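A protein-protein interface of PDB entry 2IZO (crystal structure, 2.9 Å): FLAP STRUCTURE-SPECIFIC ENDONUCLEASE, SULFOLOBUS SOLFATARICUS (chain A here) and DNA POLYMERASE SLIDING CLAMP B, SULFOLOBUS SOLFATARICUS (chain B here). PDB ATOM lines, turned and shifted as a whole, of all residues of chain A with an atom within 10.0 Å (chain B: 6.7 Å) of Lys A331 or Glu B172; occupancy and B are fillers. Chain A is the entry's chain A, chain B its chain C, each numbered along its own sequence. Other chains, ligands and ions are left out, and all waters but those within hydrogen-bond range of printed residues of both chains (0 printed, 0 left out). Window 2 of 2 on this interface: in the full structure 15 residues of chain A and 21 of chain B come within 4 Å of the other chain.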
ATOM      1  N   LEU A  66       8.896  -2.890  23.175  1.00  0.00           N
ATOM      2  CA  LEU A  66       9.355  -2.495  21.840  1.00  0.00           C
ATOM      3  C   LEU A  66       9.490  -3.676  20.882  1.00  0.00           C
ATOM      4  O   LEU A  66       9.248  -3.533  19.682  1.00  0.00           O
ATOM      5  CB  LEU A  66      10.691  -1.748  21.929  1.00  0.00           C
ATOM      6  CG  LEU A  66      10.678  -0.250  22.236  1.00  0.00           C
ATOM      7  CD1 LEU A  66      11.940   0.150  22.977  1.00  0.00           C
ATOM      8  CD2 LEU A  66      10.515   0.575  20.966  1.00  0.00           C
ATOM      9  N   GLU A  67       9.881  -4.833  21.414  1.00  0.00           N
ATOM     10  CA  GLU A  67      10.029  -6.049  20.612  1.00  0.00           C
ATOM     11  C   GLU A  67       8.672  -6.537  20.114  1.00  0.00           C
ATOM     12  O   GLU A  67       8.585  -7.277  19.131  1.00  0.00           O
ATOM     13  CB  GLU A  67      10.740  -7.142  21.412  1.00  0.00           C
ATOM     14  N   GLY A  69       6.253  -4.297  19.282  1.00  0.00           N
ATOM     15  CA  GLY A  69       5.843  -3.296  18.294  1.00  0.00           C
ATOM     16  C   GLY A  69       5.245  -2.021  18.865  1.00  0.00           C
ATOM     17  O   GLY A  69       4.890  -1.103  18.116  1.00  0.00           O
ATOM     18  N   ILE A  71       5.355   1.468  20.521  1.00  0.00           N
ATOM     19  CA  ILE A  71       6.238   2.602  20.772  1.00  0.00           C
ATOM     20  C   ILE A  71       5.824   3.253  22.093  1.00  0.00           C
ATOM     21  O   ILE A  71       4.720   3.792  22.208  1.00  0.00           O
ATOM     22  CB  ILE A  71       6.251   3.628  19.615  1.00  0.00           C
ATOM     23  CG1 ILE A  71       6.759   2.970  18.328  1.00  0.00           C
ATOM     24  CG2 ILE A  71       7.113   4.843  19.987  1.00  0.00           C
ATOM     25  CD1 ILE A  71       6.752   3.881  17.102  1.00  0.00           C
ATOM     26  N   LEU A 296      11.501   7.984  18.319  1.00  0.00           N
ATOM     27  CA  LEU A 296      12.543   7.069  18.794  1.00  0.00           C
ATOM     28  C   LEU A 296      13.928   7.437  18.263  1.00  0.00           C
ATOM     29  O   LEU A 296      14.151   7.488  17.052  1.00  0.00           O
ATOM     30  CB  LEU A 296      12.210   5.619  18.422  1.00  0.00           C
ATOM     31  CG  LEU A 296      11.145   4.860  19.222  1.00  0.00           C
ATOM     32  CD1 LEU A 296      10.769   3.567  18.508  1.00  0.00           C
ATOM     33  CD2 LEU A 296      11.606   4.572  20.653  1.00  0.00           C
ATOM     34  N   ASN A 297      14.853   7.691  19.185  1.00  0.00           N
ATOM     35  CA  ASN A 297      16.232   8.013  18.838  1.00  0.00           C
ATOM     36  C   ASN A 297      17.164   6.814  19.014  1.00  0.00           C
ATOM     37  O   ASN A 297      16.733   5.741  19.439  1.00  0.00           O
ATOM     38  CB  ASN A 297      16.719   9.213  19.661  1.00  0.00           C
ATOM     39  CG  ASN A 297      16.056  10.520  19.245  1.00  0.00           C
ATOM     40  OD1 ASN A 297      14.953  10.531  18.696  1.00  0.00           O
ATOM     41  ND2 ASN A 297      16.731  11.632  19.510  1.00  0.00           N
ATOM     42  N   GLU A 298      18.434   7.002  18.667  1.00  0.00           N
ATOM     43  CA  GLU A 298      19.450   5.962  18.813  1.00  0.00           C
ATOM     44  C   GLU A 298      19.951   5.843  20.253  1.00  0.00           C
ATOM     45  O   GLU A 298      20.409   6.833  20.835  1.00  0.00           O
ATOM     46  CB  GLU A 298      20.628   6.223  17.873  1.00  0.00           C
ATOM     47  CG  GLU A 298      20.538   5.496  16.549  1.00  0.00           C
ATOM     48  CD  GLU A 298      21.834   5.569  15.771  1.00  0.00           C
ATOM     49  OE1 GLU A 298      22.166   6.664  15.273  1.00  0.00           O
ATOM     50  OE2 GLU A 298      22.521   4.531  15.658  1.00  0.00           O
ATOM     51  N   PRO A 299      19.866   4.630  20.832  1.00  0.00           N
ATOM     52  CA  PRO A 299      20.380   4.398  22.182  1.00  0.00           C
ATOM     53  C   PRO A 299      21.904   4.284  22.211  1.00  0.00           C
ATOM     54  O   PRO A 299      22.465   3.371  21.600  1.00  0.00           O
ATOM     55  CB  PRO A 299      19.733   3.068  22.582  1.00  0.00           C
ATOM     56  CG  PRO A 299      19.458   2.366  21.300  1.00  0.00           C
ATOM     57  CD  PRO A 299      19.265   3.416  20.243  1.00  0.00           C
ATOM     58  N   GLU A 324      21.717  -4.920  22.810  1.00  0.00           N
ATOM     59  CA  GLU A 324      21.823  -5.304  21.410  1.00  0.00           C
ATOM     60  C   GLU A 324      20.442  -5.533  20.802  1.00  0.00           C
ATOM     61  O   GLU A 324      20.181  -5.106  19.675  1.00  0.00           O
ATOM     62  CB  GLU A 324      22.695  -6.551  21.258  1.00  0.00           C
ATOM     63  CG  GLU A 324      23.355  -6.683  19.891  1.00  0.00           C
ATOM     64  CD  GLU A 324      24.455  -7.728  19.866  1.00  0.00           C
ATOM     65  OE1 GLU A 324      24.253  -8.835  20.413  1.00  0.00           O
ATOM     66  OE2 GLU A 324      25.525  -7.446  19.288  1.00  0.00           O
ATOM     67  N   ARG A 325      19.558  -6.193  21.547  1.00  0.00           N
ATOM     68  CA  ARG A 325      18.191  -6.407  21.071  1.00  0.00           C
ATOM     69  C   ARG A 325      17.299  -5.171  21.227  1.00  0.00           C
ATOM     70  O   ARG A 325      16.224  -5.109  20.628  1.00  0.00           O
ATOM     71  CB  ARG A 325      17.541  -7.665  21.678  1.00  0.00           C
ATOM     72  CG  ARG A 325      17.488  -7.729  23.194  1.00  0.00           C
ATOM     73  CD  ARG A 325      16.434  -8.728  23.653  1.00  0.00           C
ATOM     74  NE  ARG A 325      16.718  -9.266  24.983  1.00  0.00           N
ATOM     75  CZ  ARG A 325      15.842  -9.928  25.736  1.00  0.00           C
ATOM     76  NH1 ARG A 325      14.602 -10.136  25.305  1.00  0.00           N
ATOM     77  NH2 ARG A 325      16.206 -10.378  26.930  1.00  0.00           N
ATOM     78  N   LEU A 326      17.749  -4.197  22.021  1.00  0.00           N
ATOM     79  CA  LEU A 326      17.042  -2.921  22.158  1.00  0.00           C
ATOM     80  C   LEU A 326      17.007  -2.192  20.819  1.00  0.00           C
ATOM     81  O   LEU A 326      15.937  -2.000  20.242  1.00  0.00           O
ATOM     82  CB  LEU A 326      17.677  -2.035  23.244  1.00  0.00           C
ATOM     83  CG  LEU A 326      17.227  -0.567  23.357  1.00  0.00           C
ATOM     84  CD1 LEU A 326      15.749  -0.437  23.737  1.00  0.00           C
ATOM     85  CD2 LEU A 326      18.098   0.194  24.344  1.00  0.00           C
ATOM     86  N   THR A 327      18.184  -1.807  20.327  1.00  0.00           N
ATOM     87  CA  THR A 327      18.311  -1.143  19.028  1.00  0.00           C
ATOM     88  C   THR A 327      17.770  -2.011  17.886  1.00  0.00           C
ATOM     89  O   THR A 327      17.217  -1.489  16.915  1.00  0.00           O
ATOM     90  CB  THR A 327      19.771  -0.678  18.744  1.00  0.00           C
ATOM     91  OG1 THR A 327      19.878  -0.199  17.396  1.00  0.00           O
ATOM     92  CG2 THR A 327      20.774  -1.810  18.962  1.00  0.00           C
ATOM     93  N   LYS A 328      17.918  -3.330  18.024  1.00  0.00           N
ATOM     94  CA  LYS A 328      17.383  -4.289  17.056  1.00  0.00           C
ATOM     95  C   LYS A 328      15.855  -4.310  17.043  1.00  0.00           C
ATOM     96  O   LYS A 328      15.248  -4.591  16.010  1.00  0.00           O
ATOM     97  CB  LYS A 328      17.930  -5.682  17.328  1.00  0.00           C
ATOM     98  N   ALA A 329      15.240  -4.013  18.188  1.00  0.00           N
ATOM     99  CA  ALA A 329      13.781  -3.967  18.292  1.00  0.00           C
ATOM    100  C   ALA A 329      13.204  -2.686  17.694  1.00  0.00           C
ATOM    101  O   ALA A 329      12.064  -2.679  17.224  1.00  0.00           O
ATOM    102  CB  ALA A 329      13.338  -4.119  19.738  1.00  0.00           C
ATOM    103  N   ILE A 330      13.992  -1.612  17.727  1.00  0.00           N
ATOM    104  CA  ILE A 330      13.600  -0.317  17.159  1.00  0.00           C
ATOM    105  C   ILE A 330      13.385  -0.411  15.641  1.00  0.00           C
ATOM    106  O   ILE A 330      12.434   0.166  15.107  1.00  0.00           O
ATOM    107  CB  ILE A 330      14.637   0.796  17.497  1.00  0.00           C
ATOM    108  CG1 ILE A 330      14.796   0.934  19.016  1.00  0.00           C
ATOM    109  CG2 ILE A 330      14.234   2.138  16.879  1.00  0.00           C
ATOM    110  CD1 ILE A 330      15.984   1.777  19.446  1.00  0.00           C
ATOM    111  N   LYS A 331      14.264  -1.152  14.963  1.00  0.00           N
ATOM    112  CA  LYS A 331      14.173  -1.360  13.514  1.00  0.00           C
ATOM    113  C   LYS A 331      12.826  -1.950  13.092  1.00  0.00           C
ATOM    114  O   LYS A 331      12.249  -1.530  12.085  1.00  0.00           O
ATOM    115  CB  LYS A 331      15.318  -2.238  13.029  1.00  0.00           C
ATOM    116  N   GLU A 332      12.333  -2.916  13.869  1.00  0.00           N
ATOM    117  CA  GLU A 332      11.031  -3.530  13.611  1.00  0.00           C
ATOM    118  C   GLU A 332       9.871  -2.702  14.159  1.00  0.00           C
ATOM    119  O   GLU A 332       8.757  -2.771  13.632  1.00  0.00           O
ATOM    120  CB  GLU A 332      10.976  -4.961  14.164  1.00  0.00           C
ATOM    121  CG  GLU A 332      11.546  -6.036  13.230  1.00  0.00           C
ATOM    122  CD  GLU A 332      10.713  -6.261  11.963  1.00  0.00           C
ATOM    123  OE1 GLU A 332      11.245  -6.873  11.012  1.00  0.00           O
ATOM    124  OE2 GLU A 332       9.535  -5.835  11.908  1.00  0.00           O
ATOM    125  N   ALA A 333      10.139  -1.928  15.213  1.00  0.00           N
ATOM    126  CA  ALA A 333       9.113  -1.107  15.872  1.00  0.00           C
ATOM    127  C   ALA A 333       8.784   0.160  15.086  1.00  0.00           C
ATOM    128  O   ALA A 333       7.611   0.472  14.868  1.00  0.00           O
ATOM    129  CB  ALA A 333       9.533  -0.760  17.296  1.00  0.00           C
ATOM    130  N   LYS A 334       9.825   0.883  14.668  1.00  0.00           N
ATOM    131  CA  LYS A 334       9.670   2.065  13.816  1.00  0.00           C
ATOM    132  C   LYS A 334       9.111   1.673  12.446  1.00  0.00           C
ATOM    133  O   LYS A 334       8.383   2.446  11.821  1.00  0.00           O
ATOM    134  CB  LYS A 334      11.001   2.813  13.669  1.00  0.00           C
ATOM    135  CG  LYS A 334      10.865   4.257  13.173  1.00  0.00           C
ATOM    136  CD  LYS A 334      12.204   5.004  13.166  1.00  0.00           C
ATOM    137  CE  LYS A 334      12.618   5.487  14.561  1.00  0.00           C
ATOM    138  NZ  LYS A 334      11.698   6.529  15.118  1.00  0.00           N
ATOM    139  N   GLY A 335       9.456   0.467  11.995  1.00  0.00           N
ATOM    140  CA  GLY A 335       8.879  -0.111  10.783  1.00  0.00           C
ATOM    141  C   GLY A 335       7.372  -0.269  10.887  1.00  0.00           C
ATOM    142  O   GLY A 335       6.630   0.208  10.025  1.00  0.00           O
ATOM    143  N   ALA A 336       6.921  -0.920  11.957  1.00  0.00           N
ATOM    144  CA  ALA A 336       5.493  -1.164  12.185  1.00  0.00           C
ATOM    145  C   ALA A 336       4.675   0.125  12.297  1.00  0.00           C
ATOM    146  O   ALA A 336       3.482   0.139  11.986  1.00  0.00           O
ATOM    147  CB  ALA A 336       5.292  -2.037  13.414  1.00  0.00           C
ATOM    148  N   SER A 337       5.328   1.198  12.740  1.00  0.00           N
ATOM    149  CA  SER A 337       4.714   2.524  12.857  1.00  0.00           C
ATOM    150  C   SER A 337       4.176   3.042  11.520  1.00  0.00           C
ATOM    151  O   SER A 337       3.171   3.754  11.481  1.00  0.00           O
ATOM    152  CB  SER A 337       5.729   3.512  13.447  1.00  0.00           C
ATOM    153  OG  SER A 337       5.556   4.830  12.949  1.00  0.00           O
ATOM    154  N   ARG A 338       4.859   2.671  10.439  1.00  0.00           N
ATOM    155  CA  ARG A 338       4.506   3.089   9.084  1.00  0.00           C
ATOM    156  C   ARG A 338       3.413   2.218   8.461  1.00  0.00           C
ATOM    157  O   ARG A 338       2.872   2.556   7.408  1.00  0.00           O
ATOM    158  CB  ARG A 338       5.750   3.046   8.191  1.00  0.00           C
ATOM    159  CG  ARG A 338       6.843   4.044   8.551  1.00  0.00           C
ATOM    160  CD  ARG A 338       8.223   3.583   8.055  1.00  0.00           C
ATOM    161  NE  ARG A 338       8.222   3.146   6.656  1.00  0.00           N
ATOM    162  CZ  ARG A 338       8.253   3.960   5.601  1.00  0.00           C
ATOM    163  NH1 ARG A 338       8.280   5.278   5.762  1.00  0.00           N
ATOM    164  NH2 ARG A 338       8.251   3.454   4.375  1.00  0.00           N
ATOM    165  N   GLN A 339       3.098   1.103   9.121  1.00  0.00           N
ATOM    166  CA  GLN A 339       2.178   0.094   8.590  1.00  0.00           C
ATOM    167  C   GLN A 339       0.734   0.568   8.514  1.00  0.00           C
ATOM    168  O   GLN A 339       0.173   1.061   9.494  1.00  0.00           O
ATOM    169  CB  GLN A 339       2.266  -1.206   9.401  1.00  0.00           C
ATOM    170  CG  GLN A 339       1.395  -2.352   8.878  1.00  0.00           C
ATOM    171  CD  GLN A 339       1.869  -2.916   7.543  1.00  0.00           C
ATOM    172  OE1 GLN A 339       3.017  -3.345   7.404  1.00  0.00           O
ATOM    173  NE2 GLN A 339       0.976  -2.928   6.559  1.00  0.00           N
ATOM    174  N   THR B 151      14.103 -10.617   3.313  1.00  0.00           N
ATOM    175  CA  THR B 151      14.071 -10.769   4.772  1.00  0.00           C
ATOM    176  C   THR B 151      15.471 -10.948   5.359  1.00  0.00           C
ATOM    177  O   THR B 151      15.696 -10.691   6.544  1.00  0.00           O
ATOM    178  CB  THR B 151      13.165 -11.938   5.221  1.00  0.00           C
ATOM    179  OG1 THR B 151      13.530 -13.128   4.515  1.00  0.00           O
ATOM    180  CG2 THR B 151      11.705 -11.623   4.953  1.00  0.00           C
ATOM    181  N   LEU B 152      16.404 -11.384   4.516  1.00  0.00           N
ATOM    182  CA  LEU B 152      17.802 -11.542   4.906  1.00  0.00           C
ATOM    183  C   LEU B 152      18.509 -10.196   5.056  1.00  0.00           C
ATOM    184  O   LEU B 152      19.431 -10.054   5.859  1.00  0.00           O
ATOM    185  CB  LEU B 152      18.539 -12.390   3.867  1.00  0.00           C
ATOM    186  CG  LEU B 152      20.025 -12.660   4.092  1.00  0.00           C
ATOM    187  CD1 LEU B 152      20.219 -13.825   5.051  1.00  0.00           C
ATOM    188  CD2 LEU B 152      20.710 -12.923   2.762  1.00  0.00           C
ATOM    189  N   VAL B 153      18.067  -9.214   4.278  1.00  0.00           N
ATOM    190  CA  VAL B 153      18.736  -7.921   4.206  1.00  0.00           C
ATOM    191  C   VAL B 153      18.081  -6.856   5.101  1.00  0.00           C
ATOM    192  O   VAL B 153      18.782  -6.079   5.764  1.00  0.00           O
ATOM    193  CB  VAL B 153      18.863  -7.459   2.729  1.00  0.00           C
ATOM    194  CG1 VAL B 153      19.309  -6.017   2.631  1.00  0.00           C
ATOM    195  CG2 VAL B 153      19.845  -8.356   1.987  1.00  0.00           C
ATOM    196  N   GLY B 154      16.750  -6.838   5.140  1.00  0.00           N
ATOM    197  CA  GLY B 154      16.023  -5.875   5.971  1.00  0.00           C
ATOM    198  C   GLY B 154      14.611  -6.264   6.378  1.00  0.00           C
ATOM    199  O   GLY B 154      14.170  -7.394   6.153  1.00  0.00           O
ATOM    200  N   GLU B 155      13.908  -5.309   6.983  1.00  0.00           N
ATOM    201  CA  GLU B 155      12.537  -5.514   7.446  1.00  0.00           C
ATOM    202  C   GLU B 155      11.510  -5.054   6.418  1.00  0.00           C
ATOM    203  O   GLU B 155      10.350  -5.471   6.458  1.00  0.00           O
ATOM    204  CB  GLU B 155      12.314  -4.789   8.770  1.00  0.00           C
ATOM    205  N   GLU B 156      11.945  -4.200   5.494  1.00  0.00           N
ATOM    206  CA  GLU B 156      11.039  -3.562   4.553  1.00  0.00           C
ATOM    207  C   GLU B 156      11.417  -3.848   3.106  1.00  0.00           C
ATOM    208  O   GLU B 156      12.592  -3.841   2.748  1.00  0.00           O
ATOM    209  CB  GLU B 156      11.002  -2.055   4.811  1.00  0.00           C
ATOM    210  CG  GLU B 156       9.794  -1.353   4.225  1.00  0.00           C
ATOM    211  CD  GLU B 156       9.327  -0.185   5.069  1.00  0.00           C
ATOM    212  OE1 GLU B 156       9.415  -0.271   6.313  1.00  0.00           O
ATOM    213  OE2 GLU B 156       8.855   0.818   4.492  1.00  0.00           O
ATOM    214  N   ALA B 170      15.397  -3.815  -1.181  1.00  0.00           N
ATOM    215  CA  ALA B 170      15.402  -3.926   0.266  1.00  0.00           C
ATOM    216  C   ALA B 170      16.737  -3.354   0.721  1.00  0.00           C
ATOM    217  O   ALA B 170      17.609  -3.096  -0.110  1.00  0.00           O
ATOM    218  CB  ALA B 170      15.262  -5.377   0.685  1.00  0.00           C
ATOM    219  N   GLY B 171      16.900  -3.140   2.024  1.00  0.00           N
ATOM    220  CA  GLY B 171      18.156  -2.613   2.541  1.00  0.00           C
ATOM    221  C   GLY B 171      17.988  -1.649   3.692  1.00  0.00           C
ATOM    222  O   GLY B 171      17.258  -0.661   3.584  1.00  0.00           O
ATOM    223  N   GLU B 172      18.683  -1.932   4.789  1.00  0.00           N
ATOM    224  CA  GLU B 172      18.535  -1.152   6.007  1.00  0.00           C
ATOM    225  C   GLU B 172      19.522   0.009   6.087  1.00  0.00           C
ATOM    226  O   GLU B 172      19.115   1.170   5.999  1.00  0.00           O
ATOM    227  CB  GLU B 172      18.647  -2.049   7.246  1.00  0.00           C
ATOM    228  CG  GLU B 172      17.427  -2.933   7.486  1.00  0.00           C
ATOM    229  CD  GLU B 172      17.364  -3.487   8.903  1.00  0.00           C
ATOM    230  OE1 GLU B 172      17.349  -2.683   9.866  1.00  0.00           O
ATOM    231  OE2 GLU B 172      17.318  -4.729   9.055  1.00  0.00           O
ATOM    232  N   GLU B 173      20.808  -0.302   6.239  1.00  0.00           N
ATOM    233  CA  GLU B 173      21.831   0.723   6.457  1.00  0.00           C
ATOM    234  C   GLU B 173      23.033   0.562   5.516  1.00  0.00           C
ATOM    235  O   GLU B 173      24.069   0.001   5.893  1.00  0.00           O
ATOM    236  CB  GLU B 173      22.276   0.723   7.927  1.00  0.00           C
ATOM    237  CG  GLU B 173      23.219   1.862   8.320  1.00  0.00           C
ATOM    238  CD  GLU B 173      24.104   1.508   9.504  1.00  0.00           C
ATOM    239  OE1 GLU B 173      25.212   2.080   9.616  1.00  0.00           O
ATOM    240  OE2 GLU B 173      23.694   0.653  10.319  1.00  0.00           O
ATOM    241  N   GLY B 174      22.884   1.055   4.288  1.00  0.00           N
ATOM    242  CA  GLY B 174      23.964   1.020   3.303  1.00  0.00           C
ATOM    243  C   GLY B 174      24.144  -0.336   2.644  1.00  0.00           C
ATOM    244  O   GLY B 174      24.767  -0.437   1.584  1.00  0.00           O
ATOM    245  N   LYS B 175      23.608  -1.379   3.275  1.00  0.00           N
ATOM    246  CA  LYS B 175      23.653  -2.721   2.709  1.00  0.00           C
ATOM    247  C   LYS B 175      22.306  -3.094   2.088  1.00  0.00           C
ATOM    248  O   LYS B 175      21.330  -3.347   2.796  1.00  0.00           O
ATOM    249  CB  LYS B 175      24.169  -3.760   3.723  1.00  0.00           C
ATOM    250  CG  LYS B 175      23.271  -4.075   4.908  1.00  0.00           C
ATOM    251  CD  LYS B 175      23.827  -5.263   5.696  1.00  0.00           C
ATOM    252  CE  LYS B 175      22.707  -6.106   6.307  1.00  0.00           C
ATOM    253  NZ  LYS B 175      23.224  -7.367   6.911  1.00  0.00           N
ATOM    254  N   ARG B 176      22.273  -3.110   0.757  1.00  0.00           N
ATOM    255  CA  ARG B 176      21.020  -3.176   0.001  1.00  0.00           C
ATOM    256  C   ARG B 176      20.830  -4.483  -0.771  1.00  0.00           C
ATOM    257  O   ARG B 176      21.742  -5.310  -0.869  1.00  0.00           O
ATOM    258  CB  ARG B 176      20.920  -1.990  -0.979  1.00  0.00           C
ATOM    259  CG  ARG B 176      21.152  -0.587  -0.386  1.00  0.00           C
ATOM    260  CD  ARG B 176      19.992  -0.078   0.482  1.00  0.00           C
ATOM    261  NE  ARG B 176      18.676  -0.331  -0.113  1.00  0.00           N
ATOM    262  CZ  ARG B 176      17.529   0.188   0.324  1.00  0.00           C
ATOM    263  NH1 ARG B 176      17.510   1.014   1.364  1.00  0.00           N
ATOM    264  NH2 ARG B 176      16.392  -0.115  -0.291  1.00  0.00           N
ATOM    265  N   ARG B 248       3.258  -0.040   3.545  1.00  0.00           N
ATOM    266  CA  ARG B 248       3.769   0.878   4.557  1.00  0.00           C
ATOM    267  C   ARG B 248       3.862   2.285   3.980  1.00  0.00           C
ATOM    268  O   ARG B 248       4.142   2.452   2.793  1.00  0.00           O
ATOM    269  CB  ARG B 248       5.114   0.397   5.097  1.00  0.00           C
ATOM    270  CG  ARG B 248       4.948  -0.713   6.112  1.00  0.00           C
ATOM    271  CD  ARG B 248       6.262  -1.274   6.583  1.00  0.00           C
ATOM    272  NE  ARG B 248       6.045  -2.309   7.589  1.00  0.00           N
ATOM    273  CZ  ARG B 248       7.009  -2.881   8.303  1.00  0.00           C
ATOM    274  NH1 ARG B 248       8.279  -2.528   8.130  1.00  0.00           N
ATOM    275  NH2 ARG B 248       6.702  -3.812   9.197  1.00  0.00           N
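OE1 of Glu B156 lies within salt-bridge range of NH1 of Arg B248.
Ile A330 touches none of the printed residues of chain B. Lys A331 touches just one residue of chain B: Glu B172. Printed residues of chain B within 4 Å of Arg A338: Glu B156 (2.7 Å) and Arg B248 (3.4 Å). Printed residues of chain B within 4 Å of Gln A339: Arg B248. No residue of chain A comes within 4 Å of Gly B154. Of the printed residues of chain A, Glu B172 touches Lys A331 (3.8 Å). The nearest residue of chain B that does not touch Lys A331 is Glu B155 (4.6 Å). The nearest residue of chain A that does not touch Glu B172 is Glu A332 (6.4 Å).
OE1 of Glu B172 touches CB of Lys A331, 3.8 Å away. Glu B155 touches Glu A332. Gly A335 touches Arg B248 (O to NE, 3.6 Å). O of Arg A338 touches CA of Arg B248, at 3.4 Å.
The side-chain carboxylate (OE2) of Glu B156 is in salt-bridge range of the guanidinium group (NH2) of Arg A338 (2.7 Å). The side-chain amide oxygen (OE1) of Gln A339 sits at hydrogen-bond distance from the guanidinium group (NE) of Arg B248 (3.2 Å).
Among the printed residues, 6 pairs touch across the chains. Among the printed residues, Asp or Glu carboxylates within 4 Å of a Lys or Arg side-chain nitrogen of the other chain: Arg A338 with Glu B156 (2.7 Å).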
